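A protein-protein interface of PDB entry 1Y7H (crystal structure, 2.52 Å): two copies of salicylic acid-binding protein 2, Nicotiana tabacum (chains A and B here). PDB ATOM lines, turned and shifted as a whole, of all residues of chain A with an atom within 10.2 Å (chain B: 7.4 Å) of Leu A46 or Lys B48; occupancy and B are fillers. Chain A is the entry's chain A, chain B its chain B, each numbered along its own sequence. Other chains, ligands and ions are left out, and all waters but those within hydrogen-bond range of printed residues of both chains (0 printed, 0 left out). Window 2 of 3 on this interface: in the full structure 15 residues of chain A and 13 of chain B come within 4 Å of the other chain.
Printed residues of chain B that touch a printed residue of chain A: Leu B46, Lys B48 and Arg B177. Along chain A the printed residues that touch a printed residue of chain B span positions 46 to 177. Among the printed residues, no Asp or Glu carboxylate lies within 4 Å of a Lys or Arg side-chain nitrogen of the other chain.
Among the printed residues, merely in contact across the chains: Leu A46 with Lys B48, Leu A46 with Arg B177, Lys A48 with Leu B46, Arg A177 with Leu B46 and Leu A46 with Leu B46.
The backbone carbonyl oxygen of Arg A47 is in hydrogen-bond range of the guanidinium group of Arg A177. The side-chain carboxylate of Glu A51 lies within hydrogen-bond range of the backbone NH of Lys A48 (3.2 Å). NH1 of Arg B177 lies within hydrogen-bond range of O of Ala B41 (3.2 Å). O of Asp B45 is in hydrogen-bond range of NH1 of Arg B177 (3.0 Å). The backbone carbonyl oxygen of Arg B47 lies within hydrogen-bond range of the guanidinium group of Arg B177 (3.4 Å). N of Lys B48 lies close to OE1 of Glu B51.
Ala A40 touches none of the printed residues of chain B. Leu A46 touches three residues of chain B. Printed residues of chain B within 4 Å of Lys A48: Leu B46 (3.4 Å). No residue of chain A comes within 4 Å of Ala B41. Printed residues of chain A within 4 Å of Leu B46: Leu A46 (3.7 Å), Lys A48 (3.4 Å) and Arg A177 (3.5 Å). No residue of chain A comes within 4 Å of Glu B50. No residue of chain A comes within 4 Å of Glu B51. The nearest residue of chain A that does not touch Lys B48 is Arg A47 (5.7 Å).
Leu B46 touches its own counterpart, Leu A46. Leu A46 touches Lys B48, and with the chains exchanged Lys A48 touches Leu B46. Leu A46 touches Arg B177, and with the chains exchanged Arg A177 touches Leu B46. 14 positions are printed for both chains. Of the 5 pairs that touch across the chains among the printed residues, 5 have their exchanged pair printed and touching as well.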
ATOM      1  N   ASP A  38     -12.194  19.241 -17.336  1.00  0.00           N
ATOM      2  CA  ASP A  38     -13.062  19.923 -16.406  1.00  0.00           C
ATOM      3  C   ASP A  38     -12.951  21.431 -16.582  1.00  0.00           C
ATOM      4  O   ASP A  38     -11.861  22.006 -16.560  1.00  0.00           O
ATOM      5  CB  ASP A  38     -12.713  19.508 -14.976  1.00  0.00           C
ATOM      6  CG  ASP A  38     -13.577  18.362 -14.484  1.00  0.00           C
ATOM      7  OD1 ASP A  38     -14.771  18.598 -14.207  1.00  0.00           O
ATOM      8  OD2 ASP A  38     -13.069  17.226 -14.388  1.00  0.00           O
ATOM      9  N   LEU A  39     -14.093  22.059 -16.798  1.00  0.00           N
ATOM     10  CA  LEU A  39     -14.142  23.497 -16.962  1.00  0.00           C
ATOM     11  C   LEU A  39     -13.990  24.155 -15.600  1.00  0.00           C
ATOM     12  O   LEU A  39     -14.125  23.507 -14.557  1.00  0.00           O
ATOM     13  CB  LEU A  39     -15.479  23.914 -17.571  1.00  0.00           C
ATOM     14  CG  LEU A  39     -15.778  23.302 -18.930  1.00  0.00           C
ATOM     15  CD1 LEU A  39     -17.101  23.816 -19.467  1.00  0.00           C
ATOM     16  CD2 LEU A  39     -14.635  23.639 -19.869  1.00  0.00           C
ATOM     17  N   ALA A  40     -13.727  25.454 -15.619  1.00  0.00           N
ATOM     18  CA  ALA A  40     -13.574  26.223 -14.393  1.00  0.00           C
ATOM     19  C   ALA A  40     -14.810  26.086 -13.490  1.00  0.00           C
ATOM     20  O   ALA A  40     -15.943  26.034 -13.975  1.00  0.00           O
ATOM     21  CB  ALA A  40     -13.335  27.670 -14.739  1.00  0.00           C
ATOM     22  N   ALA A  41     -14.575  26.024 -12.179  1.00  0.00           N
ATOM     23  CA  ALA A  41     -15.627  25.874 -11.168  1.00  0.00           C
ATOM     24  C   ALA A  41     -16.466  24.602 -11.369  1.00  0.00           C
ATOM     25  O   ALA A  41     -17.603  24.511 -10.907  1.00  0.00           O
ATOM     26  CB  ALA A  41     -16.519  27.114 -11.147  1.00  0.00           C
ATOM     27  N   SER A  42     -15.879  23.619 -12.047  1.00  0.00           N
ATOM     28  CA  SER A  42     -16.532  22.338 -12.337  1.00  0.00           C
ATOM     29  C   SER A  42     -15.709  21.146 -11.820  1.00  0.00           C
ATOM     30  O   SER A  42     -14.482  21.216 -11.751  1.00  0.00           O
ATOM     31  CB  SER A  42     -16.717  22.202 -13.844  1.00  0.00           C
ATOM     32  OG  SER A  42     -17.341  23.354 -14.374  1.00  0.00           O
ATOM     33  N   GLY A  43     -16.381  20.052 -11.472  1.00  0.00           N
ATOM     34  CA  GLY A  43     -15.665  18.892 -10.980  1.00  0.00           C
ATOM     35  C   GLY A  43     -14.716  19.253  -9.855  1.00  0.00           C
ATOM     36  O   GLY A  43     -15.149  19.759  -8.819  1.00  0.00           O
ATOM     37  N   THR A  44     -13.419  19.021 -10.053  1.00  0.00           N
ATOM     38  CA  THR A  44     -12.425  19.323  -9.014  1.00  0.00           C
ATOM     39  C   THR A  44     -11.670  20.652  -9.166  1.00  0.00           C
ATOM     40  O   THR A  44     -10.634  20.852  -8.528  1.00  0.00           O
ATOM     41  CB  THR A  44     -11.356  18.215  -8.903  1.00  0.00           C
ATOM     42  OG1 THR A  44     -10.447  18.310 -10.007  1.00  0.00           O
ATOM     43  CG2 THR A  44     -12.004  16.841  -8.888  1.00  0.00           C
ATOM     44  N   ASP A  45     -12.162  21.557 -10.003  1.00  0.00           N
ATOM     45  CA  ASP A  45     -11.483  22.836 -10.166  1.00  0.00           C
ATOM     46  C   ASP A  45     -11.708  23.611  -8.865  1.00  0.00           C
ATOM     47  O   ASP A  45     -12.769  23.499  -8.246  1.00  0.00           O
ATOM     48  CB  ASP A  45     -12.056  23.596 -11.366  1.00  0.00           C
ATOM     49  CG  ASP A  45     -11.107  24.667 -11.896  1.00  0.00           C
ATOM     50  OD1 ASP A  45      -9.948  24.320 -12.215  1.00  0.00           O
ATOM     51  OD2 ASP A  45     -11.524  25.846 -12.003  1.00  0.00           O
ATOM     52  N   LEU A  46     -10.711  24.387  -8.452  1.00  0.00           N
ATOM     53  CA  LEU A  46     -10.788  25.134  -7.203  1.00  0.00           C
ATOM     54  C   LEU A  46     -11.425  26.504  -7.313  1.00  0.00           C
ATOM     55  O   LEU A  46     -11.741  27.130  -6.303  1.00  0.00           O
ATOM     56  CB  LEU A  46      -9.392  25.262  -6.591  1.00  0.00           C
ATOM     57  CG  LEU A  46      -8.719  23.916  -6.292  1.00  0.00           C
ATOM     58  CD1 LEU A  46      -7.406  24.145  -5.555  1.00  0.00           C
ATOM     59  CD2 LEU A  46      -9.655  23.051  -5.458  1.00  0.00           C
ATOM     60  N   ARG A  47     -11.604  26.980  -8.539  1.00  0.00           N
ATOM     61  CA  ARG A  47     -12.237  28.271  -8.736  1.00  0.00           C
ATOM     62  C   ARG A  47     -13.713  28.145  -8.345  1.00  0.00           C
ATOM     63  O   ARG A  47     -14.281  27.050  -8.376  1.00  0.00           O
ATOM     64  CB  ARG A  47     -12.092  28.711 -10.204  1.00  0.00           C
ATOM     65  CG  ARG A  47     -10.668  29.139 -10.592  1.00  0.00           C
ATOM     66  CD  ARG A  47     -10.475  29.307 -12.102  1.00  0.00           C
ATOM     67  NE  ARG A  47     -10.347  28.020 -12.788  1.00  0.00           N
ATOM     68  CZ  ARG A  47      -9.547  27.793 -13.828  1.00  0.00           C
ATOM     69  NH1 ARG A  47      -8.790  28.768 -14.318  1.00  0.00           N
ATOM     70  NH2 ARG A  47      -9.493  26.585 -14.378  1.00  0.00           N
ATOM     71  N   LYS A  48     -14.315  29.265  -7.950  1.00  0.00           N
ATOM     72  CA  LYS A  48     -15.727  29.315  -7.574  1.00  0.00           C
ATOM     73  C   LYS A  48     -16.507  29.991  -8.693  1.00  0.00           C
ATOM     74  O   LYS A  48     -15.966  30.811  -9.438  1.00  0.00           O
ATOM     75  CB  LYS A  48     -15.931  30.118  -6.285  1.00  0.00           C
ATOM     76  CG  LYS A  48     -15.254  29.526  -5.051  1.00  0.00           C
ATOM     77  CD  LYS A  48     -15.875  30.064  -3.756  1.00  0.00           C
ATOM     78  CE  LYS A  48     -15.240  29.414  -2.538  1.00  0.00           C
ATOM     79  NZ  LYS A  48     -15.833  29.846  -1.250  1.00  0.00           N
ATOM     80  N   ILE A  49     -17.786  29.653  -8.798  1.00  0.00           N
ATOM     81  CA  ILE A  49     -18.629  30.224  -9.830  1.00  0.00           C
ATOM     82  C   ILE A  49     -18.729  31.743  -9.691  1.00  0.00           C
ATOM     83  O   ILE A  49     -19.178  32.414 -10.616  1.00  0.00           O
ATOM     84  CB  ILE A  49     -20.052  29.572  -9.810  1.00  0.00           C
ATOM     85  CG1 ILE A  49     -20.812  29.899 -11.090  1.00  0.00           C
ATOM     86  CG2 ILE A  49     -20.851  30.102  -8.647  1.00  0.00           C
ATOM     87  CD1 ILE A  49     -20.137  29.427 -12.361  1.00  0.00           C
ATOM     88  N   GLU A  50     -18.309  32.292  -8.550  1.00  0.00           N
ATOM     89  CA  GLU A  50     -18.353  33.744  -8.370  1.00  0.00           C
ATOM     90  C   GLU A  50     -17.232  34.441  -9.121  1.00  0.00           C
ATOM     91  O   GLU A  50     -17.362  35.601  -9.483  1.00  0.00           O
ATOM     92  CB  GLU A  50     -18.262  34.153  -6.898  1.00  0.00           C
ATOM     93  CG  GLU A  50     -19.495  33.841  -6.090  1.00  0.00           C
ATOM     94  CD  GLU A  50     -19.666  32.357  -5.908  1.00  0.00           C
ATOM     95  OE1 GLU A  50     -18.659  31.699  -5.563  1.00  0.00           O
ATOM     96  OE2 GLU A  50     -20.794  31.862  -6.099  1.00  0.00           O
ATOM     97  N   GLU A  51     -16.127  33.750  -9.349  1.00  0.00           N
ATOM     98  CA  GLU A  51     -15.021  34.374 -10.065  1.00  0.00           C
ATOM     99  C   GLU A  51     -15.266  34.279 -11.566  1.00  0.00           C
ATOM    100  O   GLU A  51     -14.394  34.598 -12.364  1.00  0.00           O
ATOM    101  CB  GLU A  51     -13.703  33.678  -9.717  1.00  0.00           C
ATOM    102  CG  GLU A  51     -13.651  33.210  -8.280  1.00  0.00           C
ATOM    103  CD  GLU A  51     -12.459  32.322  -7.967  1.00  0.00           C
ATOM    104  OE1 GLU A  51     -12.510  31.666  -6.902  1.00  0.00           O
ATOM    105  OE2 GLU A  51     -11.489  32.294  -8.765  1.00  0.00           O
ATOM    106  N   LEU A  52     -16.449  33.829 -11.953  1.00  0.00           N
ATOM    107  CA  LEU A  52     -16.735  33.705 -13.370  1.00  0.00           C
ATOM    108  C   LEU A  52     -17.814  34.704 -13.750  1.00  0.00           C
ATOM    109  O   LEU A  52     -18.830  34.804 -13.076  1.00  0.00           O
ATOM    110  CB  LEU A  52     -17.173  32.270 -13.698  1.00  0.00           C
ATOM    111  CG  LEU A  52     -16.118  31.210 -13.356  1.00  0.00           C
ATOM    112  CD1 LEU A  52     -16.701  29.820 -13.507  1.00  0.00           C
ATOM    113  CD2 LEU A  52     -14.913  31.386 -14.233  1.00  0.00           C
ATOM    114  N   PRO A  61     -10.448  26.648 -19.547  1.00  0.00           N
ATOM    115  CA  PRO A  61      -9.791  25.328 -19.566  1.00  0.00           C
ATOM    116  C   PRO A  61      -9.807  24.668 -20.945  1.00  0.00           C
ATOM    117  O   PRO A  61      -8.832  24.033 -21.362  1.00  0.00           O
ATOM    118  CB  PRO A  61     -10.589  24.528 -18.540  1.00  0.00           C
ATOM    119  CG  PRO A  61     -11.002  25.563 -17.563  1.00  0.00           C
ATOM    120  CD  PRO A  61     -11.445  26.701 -18.462  1.00  0.00           C
ATOM    121  N   ARG A 177     -22.207  20.811  -8.981  1.00  0.00           N
ATOM    122  CA  ARG A 177     -21.791  22.089  -8.402  1.00  0.00           C
ATOM    123  C   ARG A 177     -22.531  23.229  -9.104  1.00  0.00           C
ATOM    124  O   ARG A 177     -23.087  23.052 -10.174  1.00  0.00           O
ATOM    125  CB  ARG A 177     -20.275  22.291  -8.554  1.00  0.00           C
ATOM    126  CG  ARG A 177     -19.421  21.116  -8.094  1.00  0.00           C
ATOM    127  CD  ARG A 177     -17.951  21.390  -8.385  1.00  0.00           C
ATOM    128  NE  ARG A 177     -17.589  22.722  -7.906  1.00  0.00           N
ATOM    129  CZ  ARG A 177     -16.389  23.282  -8.014  1.00  0.00           C
ATOM    130  NH1 ARG A 177     -15.378  22.637  -8.589  1.00  0.00           N
ATOM    131  NH2 ARG A 177     -16.215  24.509  -7.551  1.00  0.00           N
ATOM    132  N   ALA B  40     -12.682  17.527   4.536  1.00  0.00           N
ATOM    133  CA  ALA B  40     -12.040  18.733   4.019  1.00  0.00           C
ATOM    134  C   ALA B  40     -11.088  18.449   2.859  1.00  0.00           C
ATOM    135  O   ALA B  40     -10.447  17.398   2.806  1.00  0.00           O
ATOM    136  CB  ALA B  40     -11.307  19.457   5.138  1.00  0.00           C
ATOM    137  N   ALA B  41     -11.020  19.388   1.923  1.00  0.00           N
ATOM    138  CA  ALA B  41     -10.151  19.249   0.765  1.00  0.00           C
ATOM    139  C   ALA B  41     -10.513  18.026  -0.067  1.00  0.00           C
ATOM    140  O   ALA B  41      -9.707  17.555  -0.859  1.00  0.00           O
ATOM    141  CB  ALA B  41      -8.704  19.146   1.227  1.00  0.00           C
ATOM    142  N   SER B  42     -11.731  17.524   0.083  1.00  0.00           N
ATOM    143  CA  SER B  42     -12.117  16.338  -0.660  1.00  0.00           C
ATOM    144  C   SER B  42     -13.368  16.473  -1.506  1.00  0.00           C
ATOM    145  O   SER B  42     -14.280  17.221  -1.161  1.00  0.00           O
ATOM    146  CB  SER B  42     -12.306  15.169   0.299  1.00  0.00           C
ATOM    147  OG  SER B  42     -11.074  14.781   0.867  1.00  0.00           O
ATOM    148  N   GLY B  43     -13.412  15.722  -2.603  1.00  0.00           N
ATOM    149  CA  GLY B  43     -14.570  15.757  -3.473  1.00  0.00           C
ATOM    150  C   GLY B  43     -14.842  17.138  -4.013  1.00  0.00           C
ATOM    151  O   GLY B  43     -14.105  17.633  -4.858  1.00  0.00           O
ATOM    152  N   THR B  44     -15.892  17.780  -3.522  1.00  0.00           N
ATOM    153  CA  THR B  44     -16.214  19.110  -4.019  1.00  0.00           C
ATOM    154  C   THR B  44     -15.948  20.193  -2.989  1.00  0.00           C
ATOM    155  O   THR B  44     -16.216  21.373  -3.228  1.00  0.00           O
ATOM    156  CB  THR B  44     -17.676  19.187  -4.476  1.00  0.00           C
ATOM    157  OG1 THR B  44     -18.537  18.811  -3.397  1.00  0.00           O
ATOM    158  CG2 THR B  44     -17.898  18.250  -5.644  1.00  0.00           C
ATOM    159  N   ASP B  45     -15.418  19.796  -1.842  1.00  0.00           N
ATOM    160  CA  ASP B  45     -15.127  20.770  -0.807  1.00  0.00           C
ATOM    161  C   ASP B  45     -14.113  21.772  -1.348  1.00  0.00           C
ATOM    162  O   ASP B  45     -13.030  21.389  -1.782  1.00  0.00           O
ATOM    163  CB  ASP B  45     -14.560  20.089   0.422  1.00  0.00           C
ATOM    164  CG  ASP B  45     -14.651  20.961   1.630  1.00  0.00           C
ATOM    165  OD1 ASP B  45     -15.757  21.064   2.197  1.00  0.00           O
ATOM    166  OD2 ASP B  45     -13.629  21.569   1.995  1.00  0.00           O
ATOM    167  N   LEU B  46     -14.449  23.054  -1.301  1.00  0.00           N
ATOM    168  CA  LEU B  46     -13.569  24.080  -1.846  1.00  0.00           C
ATOM    169  C   LEU B  46     -12.306  24.407  -1.067  1.00  0.00           C
ATOM    170  O   LEU B  46     -11.537  25.270  -1.488  1.00  0.00           O
ATOM    171  CB  LEU B  46     -14.371  25.356  -2.087  1.00  0.00           C
ATOM    172  CG  LEU B  46     -15.362  25.257  -3.254  1.00  0.00           C
ATOM    173  CD1 LEU B  46     -16.489  26.260  -3.057  1.00  0.00           C
ATOM    174  CD2 LEU B  46     -14.628  25.499  -4.577  1.00  0.00           C
ATOM    175  N   ARG B  47     -12.082  23.733   0.059  1.00  0.00           N
ATOM    176  CA  ARG B  47     -10.877  23.970   0.858  1.00  0.00           C
ATOM    177  C   ARG B  47      -9.672  23.289   0.212  1.00  0.00           C
ATOM    178  O   ARG B  47      -9.782  22.153  -0.244  1.00  0.00           O
ATOM    179  CB  ARG B  47     -11.059  23.431   2.286  1.00  0.00           C
ATOM    180  CG  ARG B  47     -11.679  24.418   3.289  1.00  0.00           C
ATOM    181  CD  ARG B  47     -12.141  23.719   4.579  1.00  0.00           C
ATOM    182  NE  ARG B  47     -13.212  22.764   4.316  1.00  0.00           N
ATOM    183  CZ  ARG B  47     -13.975  22.195   5.244  1.00  0.00           C
ATOM    184  NH1 ARG B  47     -13.803  22.475   6.527  1.00  0.00           N
ATOM    185  NH2 ARG B  47     -14.925  21.337   4.884  1.00  0.00           N
ATOM    186  N   LYS B  48      -8.535  23.990   0.174  1.00  0.00           N
ATOM    187  CA  LYS B  48      -7.288  23.464  -0.392  1.00  0.00           C
ATOM    188  C   LYS B  48      -6.616  22.574   0.643  1.00  0.00           C
ATOM    189  O   LYS B  48      -6.754  22.801   1.849  1.00  0.00           O
ATOM    190  CB  LYS B  48      -6.297  24.583  -0.746  1.00  0.00           C
ATOM    191  CG  LYS B  48      -6.595  25.404  -1.992  1.00  0.00           C
ATOM    192  CD  LYS B  48      -7.533  26.565  -1.699  1.00  0.00           C
ATOM    193  CE  LYS B  48      -7.534  27.581  -2.841  1.00  0.00           C
ATOM    194  NZ  LYS B  48      -8.012  27.012  -4.138  1.00  0.00           N
ATOM    195  N   ILE B  49      -5.863  21.581   0.175  1.00  0.00           N
ATOM    196  CA  ILE B  49      -5.176  20.663   1.075  1.00  0.00           C
ATOM    197  C   ILE B  49      -4.123  21.367   1.931  1.00  0.00           C
ATOM    198  O   ILE B  49      -3.863  20.964   3.068  1.00  0.00           O
ATOM    199  CB  ILE B  49      -4.513  19.502   0.294  1.00  0.00           C
ATOM    200  CG1 ILE B  49      -3.757  18.593   1.265  1.00  0.00           C
ATOM    201  CG2 ILE B  49      -3.626  20.037  -0.812  1.00  0.00           C
ATOM    202  CD1 ILE B  49      -4.679  17.847   2.226  1.00  0.00           C
ATOM    203  N   GLU B  50      -3.530  22.422   1.383  1.00  0.00           N
ATOM    204  CA  GLU B  50      -2.514  23.190   2.089  1.00  0.00           C
ATOM    205  C   GLU B  50      -3.103  23.958   3.276  1.00  0.00           C
ATOM    206  O   GLU B  50      -2.370  24.604   4.023  1.00  0.00           O
ATOM    207  CB  GLU B  50      -1.828  24.179   1.137  1.00  0.00           C
ATOM    208  CG  GLU B  50      -1.193  23.552  -0.095  1.00  0.00           C
ATOM    209  CD  GLU B  50      -2.232  23.060  -1.092  1.00  0.00           C
ATOM    210  OE1 GLU B  50      -1.871  22.301  -2.018  1.00  0.00           O
ATOM    211  OE2 GLU B  50      -3.411  23.448  -0.943  1.00  0.00           O
ATOM    212  N   GLU B  51      -4.422  23.892   3.443  1.00  0.00           N
ATOM    213  CA  GLU B  51      -5.094  24.580   4.550  1.00  0.00           C
ATOM    214  C   GLU B  51      -5.268  23.660   5.769  1.00  0.00           C
ATOM    215  O   GLU B  51      -5.619  24.114   6.859  1.00  0.00           O
ATOM    216  CB  GLU B  51      -6.479  25.068   4.124  1.00  0.00           C
ATOM    217  CG  GLU B  51      -6.511  25.920   2.873  1.00  0.00           C
ATOM    218  CD  GLU B  51      -7.934  26.243   2.432  1.00  0.00           C
ATOM    219  OE1 GLU B  51      -8.100  26.969   1.427  1.00  0.00           O
ATOM    220  OE2 GLU B  51      -8.892  25.771   3.089  1.00  0.00           O
ATOM    221  N   LEU B  52      -5.035  22.365   5.586  1.00  0.00           N
ATOM    222  CA  LEU B  52      -5.189  21.424   6.688  1.00  0.00           C
ATOM    223  C   LEU B  52      -3.832  21.252   7.371  1.00  0.00           C
ATOM    224  O   LEU B  52      -2.877  20.774   6.763  1.00  0.00           O
ATOM    225  CB  LEU B  52      -5.737  20.082   6.162  1.00  0.00           C
ATOM    226  CG  LEU B  52      -6.820  20.127   5.067  1.00  0.00           C
ATOM    227  CD1 LEU B  52      -7.521  18.770   4.948  1.00  0.00           C
ATOM    228  CD2 LEU B  52      -7.841  21.197   5.399  1.00  0.00           C
ATOM    229  N   TYR B 139       4.502  21.043   1.992  1.00  0.00           N
ATOM    230  CA  TYR B 139       3.849  22.346   1.968  1.00  0.00           C
ATOM    231  C   TYR B 139       3.875  23.040   3.334  1.00  0.00           C
ATOM    232  O   TYR B 139       2.979  23.823   3.660  1.00  0.00           O
ATOM    233  CB  TYR B 139       2.406  22.200   1.491  1.00  0.00           C
ATOM    234  CG  TYR B 139       1.543  21.320   2.358  1.00  0.00           C
ATOM    235  CD1 TYR B 139       1.613  19.922   2.267  1.00  0.00           C
ATOM    236  CD2 TYR B 139       0.623  21.886   3.244  1.00  0.00           C
ATOM    237  CE1 TYR B 139       0.775  19.109   3.038  1.00  0.00           C
ATOM    238  CE2 TYR B 139      -0.216  21.093   4.017  1.00  0.00           C
ATOM    239  CZ  TYR B 139      -0.142  19.708   3.913  1.00  0.00           C
ATOM    240  OH  TYR B 139      -0.995  18.941   4.680  1.00  0.00           O
ATOM    241  N   ARG B 177      -8.133  13.920  -5.650  1.00  0.00           N
ATOM    242  CA  ARG B 177      -7.435  15.155  -5.317  1.00  0.00           C
ATOM    243  C   ARG B 177      -6.338  14.894  -4.299  1.00  0.00           C
ATOM    244  O   ARG B 177      -6.291  13.830  -3.684  1.00  0.00           O
ATOM    245  CB  ARG B 177      -8.407  16.170  -4.736  1.00  0.00           C
ATOM    246  CG  ARG B 177      -9.506  16.557  -5.681  1.00  0.00           C
ATOM    247  CD  ARG B 177     -10.498  17.362  -4.920  1.00  0.00           C
ATOM    248  NE  ARG B 177      -9.862  18.589  -4.450  1.00  0.00           N
ATOM    249  CZ  ARG B 177     -10.379  19.400  -3.538  1.00  0.00           C
ATOM    250  NH1 ARG B 177     -11.546  19.113  -2.982  1.00  0.00           N
ATOM    251  NH2 ARG B 177      -9.732  20.502  -3.209  1.00  0.00           N
ATOM    252  N   PRO B 178      -5.431  15.869  -4.113  1.00  0.00           N
ATOM    253  CA  PRO B 178      -4.332  15.720  -3.151  1.00  0.00           C
ATOM    254  C   PRO B 178      -4.822  15.681  -1.701  1.00  0.00           C
ATOM    255  O   PRO B 178      -5.794  16.346  -1.331  1.00  0.00           O
ATOM    256  CB  PRO B 178      -3.432  16.925  -3.454  1.00  0.00           C
ATOM    257  CG  PRO B 178      -4.376  17.929  -4.014  1.00  0.00           C
ATOM    258  CD  PRO B 178      -5.311  17.126  -4.871  1.00  0.00           C
